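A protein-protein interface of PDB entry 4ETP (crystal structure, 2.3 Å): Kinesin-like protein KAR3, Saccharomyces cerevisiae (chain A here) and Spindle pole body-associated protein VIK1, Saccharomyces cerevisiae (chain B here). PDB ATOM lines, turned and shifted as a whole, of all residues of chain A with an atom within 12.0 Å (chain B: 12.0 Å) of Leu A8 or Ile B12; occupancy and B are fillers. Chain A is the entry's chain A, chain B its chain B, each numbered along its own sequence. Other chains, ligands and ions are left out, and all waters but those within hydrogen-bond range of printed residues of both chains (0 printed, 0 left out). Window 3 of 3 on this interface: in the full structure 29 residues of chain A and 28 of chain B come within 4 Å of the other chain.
NZ of Lys A16 is in salt-bridge range of OE1 of Glu B11, 3.5 Å away. The side-chain amino group of Lys A18 is in salt-bridge range of the side-chain carboxylate of Glu B23 (3.98 Å).
Ile B12 touches Leu A8. Lys A11 touches Ile B12 (CD to CD1, 3.8 Å). Ile A12 touches Leu B8. CG2 of Ile A12 touches OE1 of Glu B11, at 3.8 Å. CD1 of Leu B15 touches O of Ile A12, at 3.97 Å. CD1 of Leu A15 touches CG2 of Ile B12, at 3.9 Å. Lys A16 touches Leu B15. CD1 of Ile B19 touches CD of Lys A18, at 3.9 Å. Ile A19 touches Ile B19 (CD1 to CG1, 3.5 Å). Ile A19 touches Leu B22.
Of chain B, only Ile B12 comes within 4 Å of Leu A8. Ile A5 touches none of the printed residues of chain B. No residue of chain B comes within 4 Å of Ala A6. No residue of chain B comes within 4 Å of Ala A7. No residue of chain B comes within 4 Å of Lys A9. Lys A11 touches just one residue of chain B: Ile B12. Leu B8 touches one residue of chain A. No residue of chain A comes within 4 Å of Glu B9. Glu B11 touches just these residues of chain A: Ile A12 and Lys A16. No residue of chain A comes within 4 Å of Ala B14. Of the printed residues of chain A, Glu B18 touches Ile A19 (3.6 Å). Of the printed residues of chain B, Lys A18 touches Ile B19 and Glu B23. Ala A13 touches none of the printed residues of chain B. The nearest residue of chain B that does not touch Leu A8 is Leu B8 (4.5 Å). The nearest residue of chain A that does not touch Ile B12 is Lys A9 (6.3 Å).
Printed residues of chain B that touch a printed residue of chain A: Leu B8, Glu B11, Ile B12, Leu B15, Glu B18, Ile B19, Leu B22 and Glu B23. Hydrophobic or aromatic side chains of chain B within 4 Å of the printed part of chain A: Leu B8, Ile B12, Leu B15, Ile B19 and Leu B22. Printed residues of chain A that touch a printed residue of chain B: Leu A8, Lys A11, Ile A12, Leu A15, Lys A16, Lys A18, Ile A19 and Leu A22. Along chain A the printed residues that touch a printed residue of chain B span positions 8 to 22. Among the printed residues, Asp or Glu carboxylates within 4 Å of a Lys or Arg side-chain nitrogen of the other chain: Lys A16 with Glu B11 and Lys A18 with Glu B23.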
ATOM      1  N   ILE A   5     -10.748  11.993  19.628  1.00  0.00           N
ATOM      2  CA  ILE A   5     -11.140  13.236  20.361  1.00  0.00           C
ATOM      3  C   ILE A   5     -11.435  12.921  21.830  1.00  0.00           C
ATOM      4  O   ILE A   5     -12.152  11.958  22.141  1.00  0.00           O
ATOM      5  CB  ILE A   5     -12.346  13.946  19.694  1.00  0.00           C
ATOM      6  CG1 ILE A   5     -12.041  14.248  18.219  1.00  0.00           C
ATOM      7  CG2 ILE A   5     -12.703  15.232  20.433  1.00  0.00           C
ATOM      8  CD1 ILE A   5     -13.263  14.552  17.370  1.00  0.00           C
ATOM      9  N   ALA A   6     -10.871  13.743  22.720  1.00  0.00           N
ATOM     10  CA  ALA A   6     -11.024  13.585  24.170  1.00  0.00           C
ATOM     11  C   ALA A   6     -12.476  13.696  24.642  1.00  0.00           C
ATOM     12  O   ALA A   6     -12.840  13.129  25.676  1.00  0.00           O
ATOM     13  CB  ALA A   6     -10.149  14.593  24.903  1.00  0.00           C
ATOM     14  N   ALA A   7     -13.290  14.427  23.880  1.00  0.00           N
ATOM     15  CA  ALA A   7     -14.720  14.586  24.159  1.00  0.00           C
ATOM     16  C   ALA A   7     -15.460  13.249  24.104  1.00  0.00           C
ATOM     17  O   ALA A   7     -16.304  12.964  24.959  1.00  0.00           O
ATOM     18  CB  ALA A   7     -15.342  15.583  23.191  1.00  0.00           C
ATOM     19  N   LEU A   8     -15.138  12.443  23.094  1.00  0.00           N
ATOM     20  CA  LEU A   8     -15.684  11.094  22.955  1.00  0.00           C
ATOM     21  C   LEU A   8     -15.138  10.189  24.055  1.00  0.00           C
ATOM     22  O   LEU A   8     -15.871   9.374  24.616  1.00  0.00           O
ATOM     23  CB  LEU A   8     -15.350  10.508  21.576  1.00  0.00           C
ATOM     24  CG  LEU A   8     -15.864  11.216  20.314  1.00  0.00           C
ATOM     25  CD1 LEU A   8     -15.076  10.767  19.092  1.00  0.00           C
ATOM     26  CD2 LEU A   8     -17.356  10.991  20.104  1.00  0.00           C
ATOM     27  N   LYS A   9     -13.851  10.356  24.364  1.00  0.00           N
ATOM     28  CA  LYS A   9     -13.165   9.587  25.403  1.00  0.00           C
ATOM     29  C   LYS A   9     -13.752   9.860  26.792  1.00  0.00           C
ATOM     30  O   LYS A   9     -13.767   8.978  27.653  1.00  0.00           O
ATOM     31  CB  LYS A   9     -11.669   9.908  25.385  1.00  0.00           C
ATOM     32  CG  LYS A   9     -10.767   8.779  25.856  1.00  0.00           C
ATOM     33  CD  LYS A   9      -9.301   9.166  25.714  1.00  0.00           C
ATOM     34  CE  LYS A   9      -8.373   7.991  25.983  1.00  0.00           C
ATOM     35  NZ  LYS A   9      -8.364   7.003  24.868  1.00  0.00           N
ATOM     36  N   GLU A  10     -14.228  11.088  26.996  1.00  0.00           N
ATOM     37  CA  GLU A  10     -14.901  11.482  28.232  1.00  0.00           C
ATOM     38  C   GLU A  10     -16.358  11.013  28.234  1.00  0.00           C
ATOM     39  O   GLU A  10     -16.942  10.783  29.298  1.00  0.00           O
ATOM     40  CB  GLU A  10     -14.830  13.001  28.413  1.00  0.00           C
ATOM     41  CG  GLU A  10     -15.203  13.498  29.803  1.00  0.00           C
ATOM     42  CD  GLU A  10     -15.274  15.013  29.889  1.00  0.00           C
ATOM     43  OE1 GLU A  10     -15.068  15.555  30.996  1.00  0.00           O
ATOM     44  OE2 GLU A  10     -15.536  15.663  28.855  1.00  0.00           O
ATOM     45  N   LYS A  11     -16.936  10.879  27.041  1.00  0.00           N
ATOM     46  CA  LYS A  11     -18.317  10.419  26.887  1.00  0.00           C
ATOM     47  C   LYS A  11     -18.449   8.930  27.214  1.00  0.00           C
ATOM     48  O   LYS A  11     -19.409   8.523  27.876  1.00  0.00           O
ATOM     49  CB  LYS A  11     -18.839  10.715  25.475  1.00  0.00           C
ATOM     50  CG  LYS A  11     -20.347  10.574  25.322  1.00  0.00           C
ATOM     51  CD  LYS A  11     -20.794  10.890  23.905  1.00  0.00           C
ATOM     52  CE  LYS A  11     -22.297  10.715  23.748  1.00  0.00           C
ATOM     53  NZ  LYS A  11     -22.749  11.005  22.359  1.00  0.00           N
ATOM     54  N   ILE A  12     -17.483   8.130  26.752  1.00  0.00           N
ATOM     55  CA  ILE A  12     -17.428   6.696  27.060  1.00  0.00           C
ATOM     56  C   ILE A  12     -17.356   6.449  28.571  1.00  0.00           C
ATOM     57  O   ILE A  12     -18.101   5.620  29.107  1.00  0.00           O
ATOM     58  CB  ILE A  12     -16.262   5.988  26.315  1.00  0.00           C
ATOM     59  CG1 ILE A  12     -16.700   5.560  24.912  1.00  0.00           C
ATOM     60  CG2 ILE A  12     -15.772   4.756  27.067  1.00  0.00           C
ATOM     61  CD1 ILE A  12     -16.148   6.419  23.796  1.00  0.00           C
ATOM     62  N   ALA A  13     -16.474   7.188  29.247  1.00  0.00           N
ATOM     63  CA  ALA A  13     -16.296   7.081  30.696  1.00  0.00           C
ATOM     64  C   ALA A  13     -17.599   7.329  31.461  1.00  0.00           C
ATOM     65  O   ALA A  13     -17.917   6.600  32.404  1.00  0.00           O
ATOM     66  CB  ALA A  13     -15.208   8.035  31.168  1.00  0.00           C
ATOM     67  N   ALA A  14     -18.347   8.351  31.040  1.00  0.00           N
ATOM     68  CA  ALA A  14     -19.630   8.699  31.657  1.00  0.00           C
ATOM     69  C   ALA A  14     -20.697   7.628  31.425  1.00  0.00           C
ATOM     70  O   ALA A  14     -21.545   7.394  32.288  1.00  0.00           O
ATOM     71  CB  ALA A  14     -20.115  10.052  31.155  1.00  0.00           C
ATOM     72  N   LEU A  15     -20.647   6.986  30.259  1.00  0.00           N
ATOM     73  CA  LEU A  15     -21.582   5.913  29.921  1.00  0.00           C
ATOM     74  C   LEU A  15     -21.282   4.641  30.713  1.00  0.00           C
ATOM     75  O   LEU A  15     -22.199   4.004  31.236  1.00  0.00           O
ATOM     76  CB  LEU A  15     -21.580   5.631  28.413  1.00  0.00           C
ATOM     77  CG  LEU A  15     -22.048   6.737  27.454  1.00  0.00           C
ATOM     78  CD1 LEU A  15     -21.705   6.376  26.017  1.00  0.00           C
ATOM     79  CD2 LEU A  15     -23.534   7.043  27.592  1.00  0.00           C
ATOM     80  N   LYS A  16     -19.999   4.287  30.808  1.00  0.00           N
ATOM     81  CA  LYS A  16     -19.550   3.132  31.594  1.00  0.00           C
ATOM     82  C   LYS A  16     -19.817   3.315  33.088  1.00  0.00           C
ATOM     83  O   LYS A  16     -20.050   2.340  33.810  1.00  0.00           O
ATOM     84  CB  LYS A  16     -18.062   2.858  31.359  1.00  0.00           C
ATOM     85  CG  LYS A  16     -17.745   2.219  30.016  1.00  0.00           C
ATOM     86  CD  LYS A  16     -16.262   1.908  29.893  1.00  0.00           C
ATOM     87  CE  LYS A  16     -15.949   1.221  28.574  1.00  0.00           C
ATOM     88  NZ  LYS A  16     -14.497   0.921  28.437  1.00  0.00           N
ATOM     89  N   GLU A  17     -19.776   4.567  33.539  1.00  0.00           N
ATOM     90  CA  GLU A  17     -20.108   4.927  34.914  1.00  0.00           C
ATOM     91  C   GLU A  17     -21.616   4.815  35.158  1.00  0.00           C
ATOM     92  O   GLU A  17     -22.048   4.389  36.233  1.00  0.00           O
ATOM     93  CB  GLU A  17     -19.622   6.347  35.213  1.00  0.00           C
ATOM     94  CG  GLU A  17     -19.621   6.731  36.684  1.00  0.00           C
ATOM     95  CD  GLU A  17     -19.073   8.127  36.921  1.00  0.00           C
ATOM     96  OE1 GLU A  17     -17.951   8.420  36.453  1.00  0.00           O
ATOM     97  OE2 GLU A  17     -19.764   8.930  37.583  1.00  0.00           O
ATOM     98  N   LYS A  18     -22.403   5.196  34.153  1.00  0.00           N
ATOM     99  CA  LYS A  18     -23.861   5.108  34.219  1.00  0.00           C
ATOM    100  C   LYS A  18     -24.329   3.650  34.226  1.00  0.00           C
ATOM    101  O   LYS A  18     -25.288   3.310  34.924  1.00  0.00           O
ATOM    102  CB  LYS A  18     -24.502   5.876  33.058  1.00  0.00           C
ATOM    103  CG  LYS A  18     -25.980   6.182  33.248  1.00  0.00           C
ATOM    104  CD  LYS A  18     -26.546   6.955  32.066  1.00  0.00           C
ATOM    105  CE  LYS A  18     -28.022   7.259  32.264  1.00  0.00           C
ATOM    106  NZ  LYS A  18     -28.599   7.995  31.106  1.00  0.00           N
ATOM    107  N   ILE A  19     -23.643   2.804  33.453  1.00  0.00           N
ATOM    108  CA  ILE A  19     -23.897   1.358  33.415  1.00  0.00           C
ATOM    109  C   ILE A  19     -23.789   0.740  34.813  1.00  0.00           C
ATOM    110  O   ILE A  19     -24.696   0.028  35.256  1.00  0.00           O
ATOM    111  CB  ILE A  19     -22.935   0.637  32.429  1.00  0.00           C
ATOM    112  CG1 ILE A  19     -23.295   0.959  30.969  1.00  0.00           C
ATOM    113  CG2 ILE A  19     -22.902  -0.873  32.668  1.00  0.00           C
ATOM    114  CD1 ILE A  19     -24.548   0.286  30.446  1.00  0.00           C
ATOM    115  N   LEU A  22     -26.648   1.909  37.058  1.00  0.00           N
ATOM    116  CA  LEU A  22     -27.928   1.267  36.758  1.00  0.00           C
ATOM    117  C   LEU A  22     -27.972  -0.189  37.226  1.00  0.00           C
ATOM    118  O   LEU A  22     -29.012  -0.660  37.691  1.00  0.00           O
ATOM    119  CB  LEU A  22     -28.257   1.357  35.263  1.00  0.00           C
ATOM    120  CG  LEU A  22     -28.491   2.740  34.642  1.00  0.00           C
ATOM    121  CD1 LEU A  22     -28.631   2.619  33.132  1.00  0.00           C
ATOM    122  CD2 LEU A  22     -29.698   3.454  35.238  1.00  0.00           C
ATOM    123  N   ALA B   6     -14.275   5.112  12.904  1.00  0.00           N
ATOM    124  CA  ALA B   6     -15.102   5.564  14.061  1.00  0.00           C
ATOM    125  C   ALA B   6     -15.364   4.416  15.037  1.00  0.00           C
ATOM    126  O   ALA B   6     -16.502   3.957  15.196  1.00  0.00           O
ATOM    127  CB  ALA B   6     -16.408   6.180  13.573  1.00  0.00           C
ATOM    128  N   ALA B   7     -14.295   3.957  15.687  1.00  0.00           N
ATOM    129  CA  ALA B   7     -14.371   2.866  16.659  1.00  0.00           C
ATOM    130  C   ALA B   7     -14.932   3.330  18.003  1.00  0.00           C
ATOM    131  O   ALA B   7     -15.657   2.585  18.667  1.00  0.00           O
ATOM    132  CB  ALA B   7     -13.003   2.222  16.844  1.00  0.00           C
ATOM    133  N   LEU B   8     -14.587   4.556  18.396  1.00  0.00           N
ATOM    134  CA  LEU B   8     -15.086   5.153  19.636  1.00  0.00           C
ATOM    135  C   LEU B   8     -16.566   5.518  19.536  1.00  0.00           C
ATOM    136  O   LEU B   8     -17.298   5.427  20.522  1.00  0.00           O
ATOM    137  CB  LEU B   8     -14.262   6.388  20.021  1.00  0.00           C
ATOM    138  CG  LEU B   8     -12.834   6.174  20.537  1.00  0.00           C
ATOM    139  CD1 LEU B   8     -12.046   7.476  20.483  1.00  0.00           C
ATOM    140  CD2 LEU B   8     -12.824   5.596  21.948  1.00  0.00           C
ATOM    141  N   GLU B   9     -16.994   5.926  18.342  1.00  0.00           N
ATOM    142  CA  GLU B   9     -18.397   6.245  18.077  1.00  0.00           C
ATOM    143  C   GLU B   9     -19.251   4.974  18.025  1.00  0.00           C
ATOM    144  O   GLU B   9     -20.435   5.000  18.369  1.00  0.00           O
ATOM    145  CB  GLU B   9     -18.528   7.035  16.770  1.00  0.00           C
ATOM    146  CG  GLU B   9     -19.831   7.810  16.628  1.00  0.00           C
ATOM    147  CD  GLU B   9     -19.902   8.623  15.347  1.00  0.00           C
ATOM    148  OE1 GLU B   9     -19.510   8.108  14.278  1.00  0.00           O
ATOM    149  OE2 GLU B   9     -20.363   9.783  15.408  1.00  0.00           O
ATOM    150  N   LYS B  10     -18.635   3.872  17.597  1.00  0.00           N
ATOM    151  CA  LYS B  10     -19.283   2.560  17.568  1.00  0.00           C
ATOM    152  C   LYS B  10     -19.471   2.007  18.983  1.00  0.00           C
ATOM    153  O   LYS B  10     -20.461   1.328  19.267  1.00  0.00           O
ATOM    154  CB  LYS B  10     -18.464   1.580  16.717  1.00  0.00           C
ATOM    155  CG  LYS B  10     -19.180   0.285  16.352  1.00  0.00           C
ATOM    156  CD  LYS B  10     -20.145   0.473  15.191  1.00  0.00           C
ATOM    157  CE  LYS B  10     -20.778  -0.845  14.778  1.00  0.00           C
ATOM    158  NZ  LYS B  10     -21.539  -1.470  15.895  1.00  0.00           N
ATOM    159  N   GLU B  11     -18.512   2.306  19.860  1.00  0.00           N
ATOM    160  CA  GLU B  11     -18.561   1.884  21.260  1.00  0.00           C
ATOM    161  C   GLU B  11     -19.650   2.629  22.035  1.00  0.00           C
ATOM    162  O   GLU B  11     -20.288   2.054  22.921  1.00  0.00           O
ATOM    163  CB  GLU B  11     -17.197   2.083  21.929  1.00  0.00           C
ATOM    164  CG  GLU B  11     -17.031   1.348  23.254  1.00  0.00           C
ATOM    165  CD  GLU B  11     -15.715   1.652  23.950  1.00  0.00           C
ATOM    166  OE1 GLU B  11     -15.637   1.437  25.178  1.00  0.00           O
ATOM    167  OE2 GLU B  11     -14.760   2.102  23.281  1.00  0.00           O
ATOM    168  N   ILE B  12     -19.854   3.903  21.694  1.00  0.00           N
ATOM    169  CA  ILE B  12     -20.915   4.726  22.288  1.00  0.00           C
ATOM    170  C   ILE B  12     -22.293   4.138  21.973  1.00  0.00           C
ATOM    171  O   ILE B  12     -23.166   4.090  22.844  1.00  0.00           O
ATOM    172  CB  ILE B  12     -20.822   6.205  21.834  1.00  0.00           C
ATOM    173  CG1 ILE B  12     -19.595   6.874  22.461  1.00  0.00           C
ATOM    174  CG2 ILE B  12     -22.077   6.984  22.218  1.00  0.00           C
ATOM    175  CD1 ILE B  12     -19.157   8.151  21.773  1.00  0.00           C
ATOM    176  N   ALA B  13     -22.469   3.683  20.732  1.00  0.00           N
ATOM    177  CA  ALA B  13     -23.700   3.018  20.302  1.00  0.00           C
ATOM    178  C   ALA B  13     -23.939   1.720  21.078  1.00  0.00           C
ATOM    179  O   ALA B  13     -25.074   1.417  21.454  1.00  0.00           O
ATOM    180  CB  ALA B  13     -23.664   2.748  18.806  1.00  0.00           C
ATOM    181  N   ALA B  14     -22.863   0.972  21.320  1.00  0.00           N
ATOM    182  CA  ALA B  14     -22.921  -0.279  22.077  1.00  0.00           C
ATOM    183  C   ALA B  14     -23.221  -0.050  23.560  1.00  0.00           C
ATOM    184  O   ALA B  14     -23.904  -0.859  24.191  1.00  0.00           O
ATOM    185  CB  ALA B  14     -21.628  -1.064  21.908  1.00  0.00           C
ATOM    186  N   LEU B  15     -22.706   1.049  24.109  1.00  0.00           N
ATOM    187  CA  LEU B  15     -22.962   1.409  25.504  1.00  0.00           C
ATOM    188  C   LEU B  15     -24.344   2.032  25.691  1.00  0.00           C
ATOM    189  O   LEU B  15     -24.959   1.877  26.749  1.00  0.00           O
ATOM    190  CB  LEU B  15     -21.875   2.345  26.045  1.00  0.00           C
ATOM    191  CG  LEU B  15     -20.502   1.736  26.356  1.00  0.00           C
ATOM    192  CD1 LEU B  15     -19.487   2.835  26.639  1.00  0.00           C
ATOM    193  CD2 LEU B  15     -20.563   0.753  27.518  1.00  0.00           C
ATOM    194  N   GLU B  16     -24.824   2.731  24.664  1.00  0.00           N
ATOM    195  CA  GLU B  16     -26.167   3.314  24.672  1.00  0.00           C
ATOM    196  C   GLU B  16     -27.238   2.228  24.534  1.00  0.00           C
ATOM    197  O   GLU B  16     -28.349   2.377  25.047  1.00  0.00           O
ATOM    198  CB  GLU B  16     -26.310   4.356  23.557  1.00  0.00           C
ATOM    199  CG  GLU B  16     -27.457   5.340  23.752  1.00  0.00           C
ATOM    200  CD  GLU B  16     -27.505   6.418  22.681  1.00  0.00           C
ATOM    201  OE1 GLU B  16     -27.747   7.591  23.035  1.00  0.00           O
ATOM    202  OE2 GLU B  16     -27.300   6.099  21.490  1.00  0.00           O
ATOM    203  N   LYS B  17     -26.893   1.143  23.840  1.00  0.00           N
ATOM    204  CA  LYS B  17     -27.784  -0.006  23.684  1.00  0.00           C
ATOM    205  C   LYS B  17     -27.917  -0.775  24.999  1.00  0.00           C
ATOM    206  O   LYS B  17     -29.001  -1.263  25.333  1.00  0.00           O
ATOM    207  CB  LYS B  17     -27.283  -0.931  22.570  1.00  0.00           C
ATOM    208  CG  LYS B  17     -28.303  -1.957  22.099  1.00  0.00           C
ATOM    209  CD  LYS B  17     -27.758  -2.802  20.959  1.00  0.00           C
ATOM    210  CE  LYS B  17     -28.792  -3.807  20.475  1.00  0.00           C
ATOM    211  NZ  LYS B  17     -28.274  -4.645  19.359  1.00  0.00           N
ATOM    212  N   GLU B  18     -26.811  -0.876  25.736  1.00  0.00           N
ATOM    213  CA  GLU B  18     -26.793  -1.562  27.026  1.00  0.00           C
ATOM    214  C   GLU B  18     -27.514  -0.750  28.103  1.00  0.00           C
ATOM    215  O   GLU B  18     -28.179  -1.321  28.969  1.00  0.00           O
ATOM    216  CB  GLU B  18     -25.357  -1.878  27.457  1.00  0.00           C
ATOM    217  CG  GLU B  18     -25.257  -2.961  28.523  1.00  0.00           C
ATOM    218  CD  GLU B  18     -23.839  -3.195  29.015  1.00  0.00           C
ATOM    219  OE1 GLU B  18     -22.893  -3.135  28.197  1.00  0.00           O
ATOM    220  OE2 GLU B  18     -23.671  -3.452  30.225  1.00  0.00           O
ATOM    221  N   ILE B  19     -27.378   0.576  28.042  1.00  0.00           N
ATOM    222  CA  ILE B  19     -28.129   1.480  28.920  1.00  0.00           C
ATOM    223  C   ILE B  19     -29.633   1.337  28.672  1.00  0.00           C
ATOM    224  O   ILE B  19     -30.418   1.270  29.621  1.00  0.00           O
ATOM    225  CB  ILE B  19     -27.673   2.955  28.762  1.00  0.00           C
ATOM    226  CG1 ILE B  19     -26.339   3.174  29.483  1.00  0.00           C
ATOM    227  CG2 ILE B  19     -28.720   3.921  29.310  1.00  0.00           C
ATOM    228  CD1 ILE B  19     -25.648   4.480  29.150  1.00  0.00           C
ATOM    229  N   ALA B  20     -30.015   1.268  27.397  1.00  0.00           N
ATOM    230  CA  ALA B  20     -31.416   1.098  27.001  1.00  0.00           C
ATOM    231  C   ALA B  20     -32.016  -0.203  27.537  1.00  0.00           C
ATOM    232  O   ALA B  20     -33.164  -0.222  27.986  1.00  0.00           O
ATOM    233  CB  ALA B  20     -31.551   1.167  25.487  1.00  0.00           C
ATOM    234  N   ALA B  21     -31.227  -1.276  27.493  1.00  0.00           N
ATOM    235  CA  ALA B  21     -31.643  -2.589  27.991  1.00  0.00           C
ATOM    236  C   ALA B  21     -31.769  -2.625  29.517  1.00  0.00           C
ATOM    237  O   ALA B  21     -32.670  -3.275  30.054  1.00  0.00           O
ATOM    238  CB  ALA B  21     -30.683  -3.668  27.509  1.00  0.00           C
ATOM    239  N   LEU B  22     -30.866  -1.927  30.204  1.00  0.00           N
ATOM    240  CA  LEU B  22     -30.884  -1.852  31.666  1.00  0.00           C
ATOM    241  C   LEU B  22     -32.012  -0.963  32.188  1.00  0.00           C
ATOM    242  O   LEU B  22     -32.647  -1.291  33.193  1.00  0.00           O
ATOM    243  CB  LEU B  22     -29.535  -1.371  32.214  1.00  0.00           C
ATOM    244  CG  LEU B  22     -28.325  -2.312  32.146  1.00  0.00           C
ATOM    245  CD1 LEU B  22     -27.069  -1.580  32.590  1.00  0.00           C
ATOM    246  CD2 LEU B  22     -28.524  -3.576  32.974  1.00  0.00           C
ATOM    247  N   GLU B  23     -32.259   0.153  31.503  1.00  0.00           N
ATOM    248  CA  GLU B  23     -33.323   1.080  31.893  1.00  0.00           C
ATOM    249  C   GLU B  23     -34.716   0.481  31.697  1.00  0.00           C
ATOM    250  O   GLU B  23     -35.638   0.782  32.460  1.00  0.00           O
ATOM    251  CB  GLU B  23     -33.196   2.412  31.148  1.00  0.00           C
ATOM    252  CG  GLU B  23     -32.132   3.337  31.727  1.00  0.00           C
ATOM    253  CD  GLU B  23     -32.006   4.654  30.979  1.00  0.00           C
ATOM    254  OE1 GLU B  23     -32.092   4.656  29.731  1.00  0.00           O
ATOM    255  OE2 GLU B  23     -31.805   5.693  31.643  1.00  0.00           O
